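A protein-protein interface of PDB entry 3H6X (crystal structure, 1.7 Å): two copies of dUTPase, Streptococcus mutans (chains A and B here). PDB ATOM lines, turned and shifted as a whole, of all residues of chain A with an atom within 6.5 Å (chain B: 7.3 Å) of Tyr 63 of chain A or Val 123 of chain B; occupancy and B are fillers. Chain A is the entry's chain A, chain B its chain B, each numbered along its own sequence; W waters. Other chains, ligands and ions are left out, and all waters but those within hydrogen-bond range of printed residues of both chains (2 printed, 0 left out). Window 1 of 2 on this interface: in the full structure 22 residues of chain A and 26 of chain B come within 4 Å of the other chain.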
ATOM      1  N   MET A  56      -1.044  -5.373  15.589  1.00  0.00           N
ATOM      2  CA  MET A  56      -0.804  -6.340  16.644  1.00  0.00           C
ATOM      3  C   MET A  56      -1.959  -7.334  16.730  1.00  0.00           C
ATOM      4  O   MET A  56      -2.982  -7.178  16.041  1.00  0.00           O
ATOM      5  CB  MET A  56      -0.624  -5.616  17.993  1.00  0.00           C
ATOM      6  CG  MET A  56      -1.818  -4.754  18.328  1.00  0.00           C
ATOM      7  SD  MET A  56      -1.342  -3.297  19.553  1.00  0.00           S
ATOM      8  CE  MET A  56       0.609  -3.350  19.394  1.00  0.00           C
ATOM      9  N   VAL A  61      -1.309  -4.682  23.232  1.00  0.00           N
ATOM     10  CA  VAL A  61      -1.278  -3.220  23.197  1.00  0.00           C
ATOM     11  C   VAL A  61       0.162  -2.759  22.970  1.00  0.00           C
ATOM     12  O   VAL A  61       1.109  -3.478  23.311  1.00  0.00           O
ATOM     13  CB  VAL A  61      -1.827  -2.622  24.525  1.00  0.00           C
ATOM     14  CG1 VAL A  61      -0.976  -3.067  25.676  1.00  0.00           C
ATOM     15  CG2 VAL A  61      -1.903  -1.097  24.465  1.00  0.00           C
ATOM     16  N   LEU A  62       0.323  -1.578  22.378  1.00  0.00           N
ATOM     17  CA  LEU A  62       1.628  -0.953  22.236  1.00  0.00           C
ATOM     18  C   LEU A  62       1.683   0.262  23.132  1.00  0.00           C
ATOM     19  O   LEU A  62       0.836   1.158  23.017  1.00  0.00           O
ATOM     20  CB  LEU A  62       1.833  -0.499  20.779  1.00  0.00           C
ATOM     21  CG  LEU A  62       3.092   0.339  20.520  1.00  0.00           C
ATOM     22  CD1 LEU A  62       4.363  -0.487  20.747  1.00  0.00           C
ATOM     23  CD2 LEU A  62       3.058   0.839  19.091  1.00  0.00           C
ATOM     24  N   TYR A  63       2.662   0.295  24.031  1.00  0.00           N
ATOM     25  CA  TYR A  63       2.861   1.470  24.877  1.00  0.00           C
ATOM     26  C   TYR A  63       4.022   2.289  24.342  1.00  0.00           C
ATOM     27  O   TYR A  63       5.055   1.723  23.950  1.00  0.00           O
ATOM     28  CB  TYR A  63       3.212   1.067  26.305  1.00  0.00           C
ATOM     29  CG  TYR A  63       2.075   0.421  27.064  1.00  0.00           C
ATOM     30  CD1 TYR A  63       0.843   1.029  27.146  1.00  0.00           C
ATOM     31  CD2 TYR A  63       2.253  -0.789  27.706  1.00  0.00           C
ATOM     32  CE1 TYR A  63      -0.206   0.440  27.845  1.00  0.00           C
ATOM     33  CE2 TYR A  63       1.205  -1.380  28.412  1.00  0.00           C
ATOM     34  CZ  TYR A  63      -0.012  -0.746  28.477  1.00  0.00           C
ATOM     35  OH  TYR A  63      -1.052  -1.315  29.173  1.00  0.00           O
ATOM     36  N   LEU A  64       3.869   3.609  24.374  1.00  0.00           N
ATOM     37  CA  LEU A  64       4.956   4.531  24.036  1.00  0.00           C
ATOM     38  C   LEU A  64       5.478   5.148  25.321  1.00  0.00           C
ATOM     39  O   LEU A  64       4.706   5.705  26.107  1.00  0.00           O
ATOM     40  CB  LEU A  64       4.459   5.665  23.129  1.00  0.00           C
ATOM     41  CG  LEU A  64       3.751   5.223  21.849  1.00  0.00           C
ATOM     42  CD1 LEU A  64       3.375   6.453  21.018  1.00  0.00           C
ATOM     43  CD2 LEU A  64       4.636   4.269  21.049  1.00  0.00           C
ATOM     44  N   PHE A  65       6.781   5.025  25.544  1.00  0.00           N
ATOM     45  CA  PHE A  65       7.407   5.642  26.705  1.00  0.00           C
ATOM     46  C   PHE A  65       8.426   6.677  26.265  1.00  0.00           C
ATOM     47  O   PHE A  65       9.036   6.573  25.195  1.00  0.00           O
ATOM     48  CB  PHE A  65       8.135   4.601  27.562  1.00  0.00           C
ATOM     49  CG  PHE A  65       7.262   3.502  28.074  1.00  0.00           C
ATOM     50  CD1 PHE A  65       6.355   3.737  29.108  1.00  0.00           C
ATOM     51  CD2 PHE A  65       7.358   2.227  27.546  1.00  0.00           C
ATOM     52  CE1 PHE A  65       5.548   2.703  29.602  1.00  0.00           C
ATOM     53  CE2 PHE A  65       6.537   1.186  28.028  1.00  0.00           C
ATOM     54  CZ  PHE A  65       5.643   1.430  29.054  1.00  0.00           C
ATOM     55  N   VAL A  82       2.482   8.164  29.060  1.00  0.00           N
ATOM     56  CA  VAL A  82       2.527   6.900  28.337  1.00  0.00           C
ATOM     57  C   VAL A  82       1.520   6.967  27.230  1.00  0.00           C
ATOM     58  O   VAL A  82       0.347   7.260  27.463  1.00  0.00           O
ATOM     59  CB  VAL A  82       2.143   5.711  29.236  1.00  0.00           C
ATOM     60  CG1 VAL A  82       2.171   4.413  28.425  1.00  0.00           C
ATOM     61  CG2 VAL A  82       3.078   5.640  30.433  1.00  0.00           C
ATOM     62  N   GLY A  83       1.976   6.683  26.016  1.00  0.00           N
ATOM     63  CA  GLY A  83       1.064   6.663  24.877  1.00  0.00           C
ATOM     64  C   GLY A  83       0.452   5.273  24.823  1.00  0.00           C
ATOM     65  O   GLY A  83       1.171   4.279  24.870  1.00  0.00           O
ATOM     66  N   VAL A  84      -0.872   5.180  24.729  1.00  0.00           N
ATOM     67  CA  VAL A  84      -1.510   3.863  24.686  1.00  0.00           C
ATOM     68  C   VAL A  84      -2.075   3.653  23.289  1.00  0.00           C
ATOM     69  O   VAL A  84      -3.109   4.226  22.948  1.00  0.00           O
ATOM     70  CB  VAL A  84      -2.634   3.736  25.739  1.00  0.00           C
ATOM     71  CG1 VAL A  84      -3.299   2.356  25.685  1.00  0.00           C
ATOM     72  CG2 VAL A  84      -2.070   3.983  27.141  1.00  0.00           C
ATOM     73  N   ILE A  85      -1.382   2.839  22.490  1.00  0.00           N
ATOM     74  CA  ILE A  85      -1.748   2.628  21.095  1.00  0.00           C
ATOM     75  C   ILE A  85      -2.488   1.314  20.955  1.00  0.00           C
ATOM     76  O   ILE A  85      -1.882   0.242  21.074  1.00  0.00           O
ATOM     77  CB  ILE A  85      -0.506   2.596  20.195  1.00  0.00           C
ATOM     78  CG1 ILE A  85       0.372   3.833  20.430  1.00  0.00           C
ATOM     79  CG2 ILE A  85      -0.895   2.452  18.749  1.00  0.00           C
ATOM     80  CD1 ILE A  85      -0.353   5.153  20.232  1.00  0.00           C
ATOM     81  N   GLN A 121      10.051   5.261  22.876  1.00  0.00           N
ATOM     82  CA  GLN A 121      10.264   3.832  22.681  1.00  0.00           C
ATOM     83  C   GLN A 121       8.947   3.102  22.818  1.00  0.00           C
ATOM     84  O   GLN A 121       8.159   3.416  23.700  1.00  0.00           O
ATOM     85  CB  GLN A 121      11.293   3.276  23.682  1.00  0.00           C
ATOM     86  CG  GLN A 121      10.969   3.524  25.128  1.00  0.00           C
ATOM     87  CD  GLN A 121      12.141   3.170  26.033  1.00  0.00           C
ATOM     88  OE1 GLN A 121      12.723   2.099  25.892  1.00  0.00           O
ATOM     89  NE2 GLN A 121      12.492   4.071  26.954  1.00  0.00           N
ATOM     90  N   GLY A 122       8.704   2.143  21.932  1.00  0.00           N
ATOM     91  CA  GLY A 122       7.440   1.422  21.930  1.00  0.00           C
ATOM     92  C   GLY A 122       7.636  -0.006  22.405  1.00  0.00           C
ATOM     93  O   GLY A 122       8.545  -0.698  21.940  1.00  0.00           O
ATOM     94  N   VAL A 123       6.770  -0.460  23.310  1.00  0.00           N
ATOM     95  CA  VAL A 123       6.843  -1.821  23.830  1.00  0.00           C
ATOM     96  C   VAL A 123       5.501  -2.512  23.621  1.00  0.00           C
ATOM     97  O   VAL A 123       4.469  -1.963  24.013  1.00  0.00           O
ATOM     98  CB  VAL A 123       7.177  -1.845  25.336  1.00  0.00           C
ATOM     99  CG1 VAL A 123       7.287  -3.296  25.854  1.00  0.00           C
ATOM    100  CG2 VAL A 123       8.475  -1.066  25.624  1.00  0.00           C
ATOM    101  N   PHE A 124       5.516  -3.702  23.011  1.00  0.00           N
ATOM    102  CA  PHE A 124       4.290  -4.485  22.833  1.00  0.00           C
ATOM    103  C   PHE A 124       4.077  -5.420  24.016  1.00  0.00           C
ATOM    104  O   PHE A 124       5.002  -6.102  24.442  1.00  0.00           O
ATOM    105  CB  PHE A 124       4.373  -5.341  21.561  1.00  0.00           C
ATOM    106  CG  PHE A 124       4.442  -4.550  20.264  1.00  0.00           C
ATOM    107  CD1 PHE A 124       3.308  -4.370  19.500  1.00  0.00           C
ATOM    108  CD2 PHE A 124       5.630  -4.038  19.798  1.00  0.00           C
ATOM    109  CE1 PHE A 124       3.349  -3.688  18.310  1.00  0.00           C
ATOM    110  CE2 PHE A 124       5.681  -3.318  18.592  1.00  0.00           C
ATOM    111  CZ  PHE A 124       4.539  -3.160  17.851  1.00  0.00           C
ATOM    112  N   MET A 125       2.846  -5.479  24.517  1.00  0.00           N
ATOM    113  CA  MET A 125       2.559  -6.289  25.709  1.00  0.00           C
ATOM    114  C   MET A 125       1.154  -6.873  25.635  1.00  0.00           C
ATOM    115  O   MET A 125       0.295  -6.335  24.927  1.00  0.00           O
ATOM    116  CB  MET A 125       2.679  -5.412  26.957  1.00  0.00           C
ATOM    117  CG  MET A 125       4.064  -4.795  27.142  1.00  0.00           C
ATOM    118  SD  MET A 125       4.011  -3.691  28.756  1.00  0.00           S
ATOM    119  CE  MET A 125       4.489  -5.117  30.018  1.00  0.00           C
ATOM    120  N   PRO A 126       0.899  -7.957  26.386  1.00  0.00           N
ATOM    121  CA  PRO A 126      -0.467  -8.493  26.487  1.00  0.00           C
ATOM    122  C   PRO A 126      -1.313  -7.685  27.471  1.00  0.00           C
ATOM    123  O   PRO A 126      -0.760  -7.105  28.407  1.00  0.00           O
ATOM    124  CB  PRO A 126      -0.246  -9.888  27.069  1.00  0.00           C
ATOM    125  CG  PRO A 126       0.994  -9.719  27.936  1.00  0.00           C
ATOM    126  CD  PRO A 126       1.872  -8.733  27.177  1.00  0.00           C
ATOM    127  N   PHE A 127      -2.624  -7.635  27.252  1.00  0.00           N
ATOM    128  CA  PHE A 127      -3.546  -7.092  28.254  1.00  0.00           C
ATOM    129  C   PHE A 127      -4.713  -8.054  28.475  1.00  0.00           C
ATOM    130  O   PHE A 127      -4.921  -8.992  27.690  1.00  0.00           O
ATOM    131  CB  PHE A 127      -4.055  -5.691  27.892  1.00  0.00           C
ATOM    132  CG  PHE A 127      -5.008  -5.663  26.734  1.00  0.00           C
ATOM    133  CD1 PHE A 127      -4.537  -5.467  25.434  1.00  0.00           C
ATOM    134  CD2 PHE A 127      -6.384  -5.813  26.935  1.00  0.00           C
ATOM    135  CE1 PHE A 127      -5.398  -5.420  24.363  1.00  0.00           C
ATOM    136  CE2 PHE A 127      -7.257  -5.767  25.857  1.00  0.00           C
ATOM    137  CZ  PHE A 127      -6.764  -5.574  24.564  1.00  0.00           C
ATOM    138  N   LEU A 128      -5.480  -7.803  29.534  1.00  0.00           N
ATOM    139  CA  LEU A 128      -6.506  -8.743  29.997  1.00  0.00           C
ATOM    140  C   LEU A 128      -7.866  -8.056  30.043  1.00  0.00           C
ATOM    141  O   LEU A 128      -7.935  -6.848  30.240  1.00  0.00           O
ATOM    142  CB  LEU A 128      -6.138  -9.273  31.378  1.00  0.00           C
ATOM    143  CG  LEU A 128      -4.785  -9.969  31.479  1.00  0.00           C
ATOM    144  CD1 LEU A 128      -4.352 -10.104  32.948  1.00  0.00           C
ATOM    145  CD2 LEU A 128      -4.875 -11.316  30.786  1.00  0.00           C
ATOM    146  N   PHE B   7     -14.440  -4.291  37.479  1.00  0.00           N
ATOM    147  CA  PHE B   7     -14.756  -3.132  38.319  1.00  0.00           C
ATOM    148  C   PHE B   7     -16.097  -3.296  38.993  1.00  0.00           C
ATOM    149  O   PHE B   7     -17.027  -3.909  38.450  1.00  0.00           O
ATOM    150  CB  PHE B   7     -14.833  -1.853  37.468  1.00  0.00           C
ATOM    151  CG  PHE B   7     -13.555  -1.523  36.765  1.00  0.00           C
ATOM    152  CD1 PHE B   7     -12.553  -0.841  37.432  1.00  0.00           C
ATOM    153  CD2 PHE B   7     -13.343  -1.910  35.446  1.00  0.00           C
ATOM    154  CE1 PHE B   7     -11.345  -0.534  36.778  1.00  0.00           C
ATOM    155  CE2 PHE B   7     -12.152  -1.610  34.802  1.00  0.00           C
ATOM    156  CZ  PHE B   7     -11.156  -0.913  35.469  1.00  0.00           C
ATOM    157  N   ALA B  27      -9.614  -2.072  22.015  1.00  0.00           N
ATOM    158  CA  ALA B  27      -8.907  -1.151  22.904  1.00  0.00           C
ATOM    159  C   ALA B  27      -8.328  -1.907  24.093  1.00  0.00           C
ATOM    160  O   ALA B  27      -8.894  -2.900  24.544  1.00  0.00           O
ATOM    161  CB  ALA B  27      -9.832  -0.065  23.385  1.00  0.00           C
ATOM    162  N   ALA B  28      -7.194  -1.422  24.591  1.00  0.00           N
ATOM    163  CA  ALA B  28      -6.543  -2.035  25.734  1.00  0.00           C
ATOM    164  C   ALA B  28      -7.182  -1.534  27.024  1.00  0.00           C
ATOM    165  O   ALA B  28      -7.220  -2.257  28.019  1.00  0.00           O
ATOM    166  CB  ALA B  28      -5.082  -1.687  25.745  1.00  0.00           C
ATOM    167  N   GLY B  29      -7.622  -0.273  26.995  1.00  0.00           N
ATOM    168  CA  GLY B  29      -8.007   0.443  28.203  1.00  0.00           C
ATOM    169  C   GLY B  29      -9.500   0.559  28.452  1.00  0.00           C
ATOM    170  O   GLY B  29     -10.296   0.639  27.509  1.00  0.00           O
ATOM    171  N   TYR B  30      -9.859   0.545  29.733  1.00  0.00           N
ATOM    172  CA  TYR B  30     -11.216   0.785  30.225  1.00  0.00           C
ATOM    173  C   TYR B  30     -11.270   2.210  30.713  1.00  0.00           C
ATOM    174  O   TYR B  30     -10.431   2.626  31.502  1.00  0.00           O
ATOM    175  CB  TYR B  30     -11.531  -0.168  31.392  1.00  0.00           C
ATOM    176  CG  TYR B  30     -11.710  -1.582  30.904  1.00  0.00           C
ATOM    177  CD1 TYR B  30     -10.617  -2.423  30.741  1.00  0.00           C
ATOM    178  CD2 TYR B  30     -12.976  -2.064  30.558  1.00  0.00           C
ATOM    179  CE1 TYR B  30     -10.776  -3.708  30.247  1.00  0.00           C
ATOM    180  CE2 TYR B  30     -13.144  -3.347  30.066  1.00  0.00           C
ATOM    181  CZ  TYR B  30     -12.039  -4.157  29.913  1.00  0.00           C
ATOM    182  OH  TYR B  30     -12.186  -5.428  29.427  1.00  0.00           O
ATOM    183  N   LEU B  32     -12.183   5.082  32.887  1.00  0.00           N
ATOM    184  CA  LEU B  32     -12.726   5.456  34.187  1.00  0.00           C
ATOM    185  C   LEU B  32     -13.228   6.898  34.138  1.00  0.00           C
ATOM    186  O   LEU B  32     -12.696   7.737  33.405  1.00  0.00           O
ATOM    187  CB  LEU B  32     -11.668   5.281  35.297  1.00  0.00           C
ATOM    188  CG  LEU B  32     -11.431   3.846  35.781  1.00  0.00           C
ATOM    189  CD1 LEU B  32     -10.590   3.055  34.793  1.00  0.00           C
ATOM    190  CD2 LEU B  32     -10.732   3.878  37.138  1.00  0.00           C
ATOM    191  N   MET B  56      -8.970  -8.443  40.761  1.00  0.00           N
ATOM    192  CA  MET B  56      -8.209  -9.128  39.717  1.00  0.00           C
ATOM    193  C   MET B  56      -7.602 -10.394  40.308  1.00  0.00           C
ATOM    194  O   MET B  56      -7.807 -10.693  41.496  1.00  0.00           O
ATOM    195  CB  MET B  56      -7.105  -8.200  39.190  1.00  0.00           C
ATOM    196  CG  MET B  56      -6.185  -7.743  40.312  1.00  0.00           C
ATOM    197  SD  MET B  56      -5.251  -6.065  39.918  1.00  0.00           S
ATOM    198  CE  MET B  56      -6.307  -5.495  38.397  1.00  0.00           C
ATOM    199  N   VAL B  61      -2.041  -6.808  37.753  1.00  0.00           N
ATOM    200  CA  VAL B  61      -2.048  -5.422  38.193  1.00  0.00           C
ATOM    201  C   VAL B  61      -2.932  -4.612  37.255  1.00  0.00           C
ATOM    202  O   VAL B  61      -3.094  -4.960  36.084  1.00  0.00           O
ATOM    203  CB  VAL B  61      -0.603  -4.855  38.226  1.00  0.00           C
ATOM    204  CG1 VAL B  61       0.003  -4.888  36.833  1.00  0.00           C
ATOM    205  CG2 VAL B  61      -0.581  -3.452  38.819  1.00  0.00           C
ATOM    206  N   LEU B  62      -3.479  -3.512  37.771  1.00  0.00           N
ATOM    207  CA  LEU B  62      -4.253  -2.578  36.968  1.00  0.00           C
ATOM    208  C   LEU B  62      -3.464  -1.282  36.901  1.00  0.00           C
ATOM    209  O   LEU B  62      -3.156  -0.695  37.941  1.00  0.00           O
ATOM    210  CB  LEU B  62      -5.607  -2.294  37.634  1.00  0.00           C
ATOM    211  CG  LEU B  62      -6.430  -1.156  36.987  1.00  0.00           C
ATOM    212  CD1 LEU B  62      -6.846  -1.486  35.572  1.00  0.00           C
ATOM    213  CD2 LEU B  62      -7.662  -0.860  37.833  1.00  0.00           C
ATOM    214  N   TYR B  63      -3.123  -0.832  35.700  1.00  0.00           N
ATOM    215  CA  TYR B  63      -2.420   0.439  35.544  1.00  0.00           C
ATOM    216  C   TYR B  63      -3.411   1.488  35.096  1.00  0.00           C
ATOM    217  O   TYR B  63      -4.290   1.200  34.276  1.00  0.00           O
ATOM    218  CB  TYR B  63      -1.366   0.333  34.447  1.00  0.00           C
ATOM    219  CG  TYR B  63      -0.173  -0.505  34.818  1.00  0.00           C
ATOM    220  CD1 TYR B  63       0.500  -0.284  36.014  1.00  0.00           C
ATOM    221  CD2 TYR B  63       0.285  -1.503  33.979  1.00  0.00           C
ATOM    222  CE1 TYR B  63       1.603  -1.059  36.364  1.00  0.00           C
ATOM    223  CE2 TYR B  63       1.382  -2.282  34.327  1.00  0.00           C
ATOM    224  CZ  TYR B  63       2.031  -2.043  35.519  1.00  0.00           C
ATOM    225  OH  TYR B  63       3.129  -2.796  35.875  1.00  0.00           O
ATOM    226  N   LEU B  64      -3.276   2.696  35.637  1.00  0.00           N
ATOM    227  CA  LEU B  64      -4.098   3.825  35.182  1.00  0.00           C
ATOM    228  C   LEU B  64      -3.219   4.759  34.383  1.00  0.00           C
ATOM    229  O   LEU B  64      -2.188   5.206  34.876  1.00  0.00           O
ATOM    230  CB  LEU B  64      -4.630   4.601  36.383  1.00  0.00           C
ATOM    231  CG  LEU B  64      -5.428   3.809  37.413  1.00  0.00           C
ATOM    232  CD1 LEU B  64      -5.919   4.755  38.505  1.00  0.00           C
ATOM    233  CD2 LEU B  64      -6.583   3.087  36.722  1.00  0.00           C
ATOM    234  N   PHE B  65      -3.611   5.022  33.140  1.00  0.00           N
ATOM    235  CA  PHE B  65      -2.873   5.944  32.283  1.00  0.00           C
ATOM    236  C   PHE B  65      -3.699   7.172  31.995  1.00  0.00           C
ATOM    237  O   PHE B  65      -4.933   7.135  31.975  1.00  0.00           O
ATOM    238  CB  PHE B  65      -2.498   5.287  30.939  1.00  0.00           C
ATOM    239  CG  PHE B  65      -1.656   4.055  31.084  1.00  0.00           C
ATOM    240  CD1 PHE B  65      -0.315   4.148  31.429  1.00  0.00           C
ATOM    241  CD2 PHE B  65      -2.207   2.804  30.874  1.00  0.00           C
ATOM    242  CE1 PHE B  65       0.463   2.997  31.566  1.00  0.00           C
ATOM    243  CE2 PHE B  65      -1.444   1.661  31.009  1.00  0.00           C
ATOM    244  CZ  PHE B  65      -0.101   1.759  31.343  1.00  0.00           C
ATOM    245  N   GLY B  83      -0.899   5.258  37.467  1.00  0.00           N
ATOM    246  CA  GLY B  83      -1.448   4.797  38.732  1.00  0.00           C
ATOM    247  C   GLY B  83      -1.268   3.288  38.778  1.00  0.00           C
ATOM    248  O   GLY B  83      -1.597   2.588  37.811  1.00  0.00           O
ATOM    249  N   GLN B 121      -7.508   5.941  31.699  1.00  0.00           N
ATOM    250  CA  GLN B 121      -7.819   4.615  31.171  1.00  0.00           C
ATOM    251  C   GLN B 121      -7.093   3.538  31.965  1.00  0.00           C
ATOM    252  O   GLN B 121      -5.929   3.689  32.313  1.00  0.00           O
ATOM    253  CB  GLN B 121      -7.462   4.515  29.700  1.00  0.00           C
ATOM    254  CG  GLN B 121      -6.040   4.844  29.367  1.00  0.00           C
ATOM    255  CD  GLN B 121      -5.841   5.016  27.859  1.00  0.00           C
ATOM    256  OE1 GLN B 121      -6.296   4.196  27.087  1.00  0.00           O
ATOM    257  NE2 GLN B 121      -5.168   6.084  27.451  1.00  0.00           N
ATOM    258  N   GLY B 122      -7.795   2.455  32.272  1.00  0.00           N
ATOM    259  CA  GLY B 122      -7.199   1.389  33.057  1.00  0.00           C
ATOM    260  C   GLY B 122      -6.937   0.152  32.207  1.00  0.00           C
ATOM    261  O   GLY B 122      -7.803  -0.280  31.447  1.00  0.00           O
ATOM    262  N   VAL B 123      -5.743  -0.419  32.350  1.00  0.00           N
ATOM    263  CA  VAL B 123      -5.357  -1.622  31.620  1.00  0.00           C
ATOM    264  C   VAL B 123      -4.926  -2.705  32.613  1.00  0.00           C
ATOM    265  O   VAL B 123      -4.093  -2.456  33.478  1.00  0.00           O
ATOM    266  CB  VAL B 123      -4.191  -1.342  30.644  1.00  0.00           C
ATOM    267  CG1 VAL B 123      -3.865  -2.603  29.836  1.00  0.00           C
ATOM    268  CG2 VAL B 123      -4.528  -0.164  29.712  1.00  0.00           C
ATOM    269  N   PHE B 124      -5.497  -3.900  32.493  1.00  0.00           N
ATOM    270  CA  PHE B 124      -5.123  -5.030  33.346  1.00  0.00           C
ATOM    271  C   PHE B 124      -4.013  -5.831  32.684  1.00  0.00           C
ATOM    272  O   PHE B 124      -4.116  -6.135  31.488  1.00  0.00           O
ATOM    273  CB  PHE B 124      -6.325  -5.965  33.518  1.00  0.00           C
ATOM    274  CG  PHE B 124      -7.453  -5.387  34.346  1.00  0.00           C
ATOM    275  CD1 PHE B 124      -7.508  -5.613  35.718  1.00  0.00           C
ATOM    276  CD2 PHE B 124      -8.458  -4.648  33.751  1.00  0.00           C
ATOM    277  CE1 PHE B 124      -8.543  -5.117  36.471  1.00  0.00           C
ATOM    278  CE2 PHE B 124      -9.513  -4.152  34.498  1.00  0.00           C
ATOM    279  CZ  PHE B 124      -9.555  -4.377  35.863  1.00  0.00           C
ATOM    280  N   MET B 125      -2.981  -6.193  33.449  1.00  0.00           N
ATOM    281  CA  MET B 125      -1.812  -6.874  32.870  1.00  0.00           C
ATOM    282  C   MET B 125      -1.224  -7.851  33.890  1.00  0.00           C
ATOM    283  O   MET B 125      -1.448  -7.698  35.083  1.00  0.00           O
ATOM    284  CB  MET B 125      -0.737  -5.858  32.458  1.00  0.00           C
ATOM    285  CG  MET B 125      -1.218  -4.856  31.422  1.00  0.00           C
ATOM    286  SD  MET B 125       0.249  -3.694  30.917  1.00  0.00           S
ATOM    287  CE  MET B 125       1.057  -4.726  29.573  1.00  0.00           C
HETATM  288  O   HOH W   1      -5.271   5.587  23.997  1.00  0.00           O
HETATM  289  O   HOH W   2      -7.260  -4.071  30.195  1.00  0.00           O
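Water W1 bridges the backbone carbonyl oxygen (O) of Val 84 of chain A (2.8 Å) and the side-chain amide nitrogen (NE2) of Gln 121 of chain B (3.5 Å).
Water W2 lies within hydrogen-bond range of O of Ala 28 of chain B (2.8 Å), O of Leu 128 of chain A (2.9 Å) and N of Phe 124 of chain B (2.9 Å).
Of the 18 printed residues of chain A, 8 touch a printed residue of chain B.
Among the printed residues, 15 pairs touch across the chains.
Among the printed residues, no Asp or Glu carboxylate lies within 4 Å of a Lys or Arg side-chain nitrogen of the other chain.
The backbone carbonyl oxygen (O) of Tyr 63 of chain A is in hydrogen-bond range of the backbone NH (N) of Val 123 of chain A.
The backbone NH (N) of Val 123 of chain B sits at hydrogen-bond distance from the backbone carbonyl oxygen (O) of Tyr 63 of chain B, 2.9 Å away.
The backbone NH (N) of Phe 65 of chain B sits at hydrogen-bond distance from the backbone carbonyl oxygen (O) of Gln 121 of chain B (2.8 Å).
N of Val 61 of chain A is in hydrogen-bond range of O of Met 125 of chain A, 2.9 Å away.
O of Met 125 of chain B sits at hydrogen-bond distance from N of Val 61 of chain B (2.9 Å).
Tyr 63 of chain A touches Phe 65 of chain B, but with the chains exchanged Phe 65 of chain A does not touch Tyr 63 of chain B (7.7 Å).
Tyr 63 of chain A touches Val 123 of chain B, but with the chains exchanged Val 123 of chain A does not touch Tyr 63 of chain B (10.4 Å).
Tyr 63 of chain A touches Met 125 of chain B, but with the chains exchanged Met 125 of chain A does not touch Tyr 63 of chain B (6.0 Å).
Met 125 of chain B touches its own counterpart, Met 125 of chain A.
Positions printed for both chains: 56, 61, 62, 63, 64, 65, 83, 121, 122, 123, 124 and 125.
Of the 15 pairs that touch across the chains among the printed residues, 1 has its exchanged pair printed and touching as well.
CG2 of Val 61 of chain A touches CB of Ala 28 of chain B (3.5 Å).
CE2 of Phe 65 of chain B touches OH of Tyr 63 of chain A, 3.5 Å away.
OH of Tyr 63 of chain A touches CG1 of Val 123 of chain B, at 3.2 Å.
CB of Val 82 of chain A touches CD1 of Phe 65 of chain B (3.6 Å).
Val 84 of chain A touches Gln 121 of chain B.
Met 125 of chain A touches Met 125 of chain B (CB to CE, 3.2 Å).
O of Ala 27 of chain B touches CZ of Phe 127 of chain A, 3.4 Å away.
CB of Phe 127 of chain A touches CG1 of Val 123 of chain B, at 3.7 Å.
O of Phe 124 of chain B touches CA of Phe 127 of chain A (3.4 Å).
C of Met 125 of chain B touches CD1 of Leu 128 of chain A, at 3.97 Å.
N of Leu 128 of chain A sits at hydrogen-bond distance from O of Phe 124 of chain B (2.9 Å).
OH of Tyr 63 of chain A lies within hydrogen-bond range of SD of Met 125 of chain B (3.2 Å).
Of chain A, only Tyr 63 (3.2 Å) and Phe 127 (3.7 Å) come within 4 Å of Val 123 of chain B.
Of the printed residues of chain A, Met 125 of chain B touches Tyr 63 (3.2 Å), Met 125 (3.2 Å), Pro 126 (3.2 Å) and Leu 128 (3.97 Å).
Printed residues of chain B within 4 Å of Val 61 of chain A: Ala 28 (3.5 Å).
Printed residues of chain B within 4 Å of Met 125 of chain A: Met 125.
Of the printed residues of chain A, Ala 27 of chain B touches Phe 127.
Of the printed residues of chain A, Phe 65 of chain B touches Tyr 63, Val 82 and Val 84.
Met 56 of chain B touches none of the printed residues of chain A.
Gly 29 of chain B touches none of the printed residues of chain A.
The nearest residue of chain B that does not touch Tyr 63 of chain A is Tyr 63 of chain B (5.0 Å).
The nearest residue of chain A that does not touch Val 123 of chain B is Val 84 of chain A (4.9 Å).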
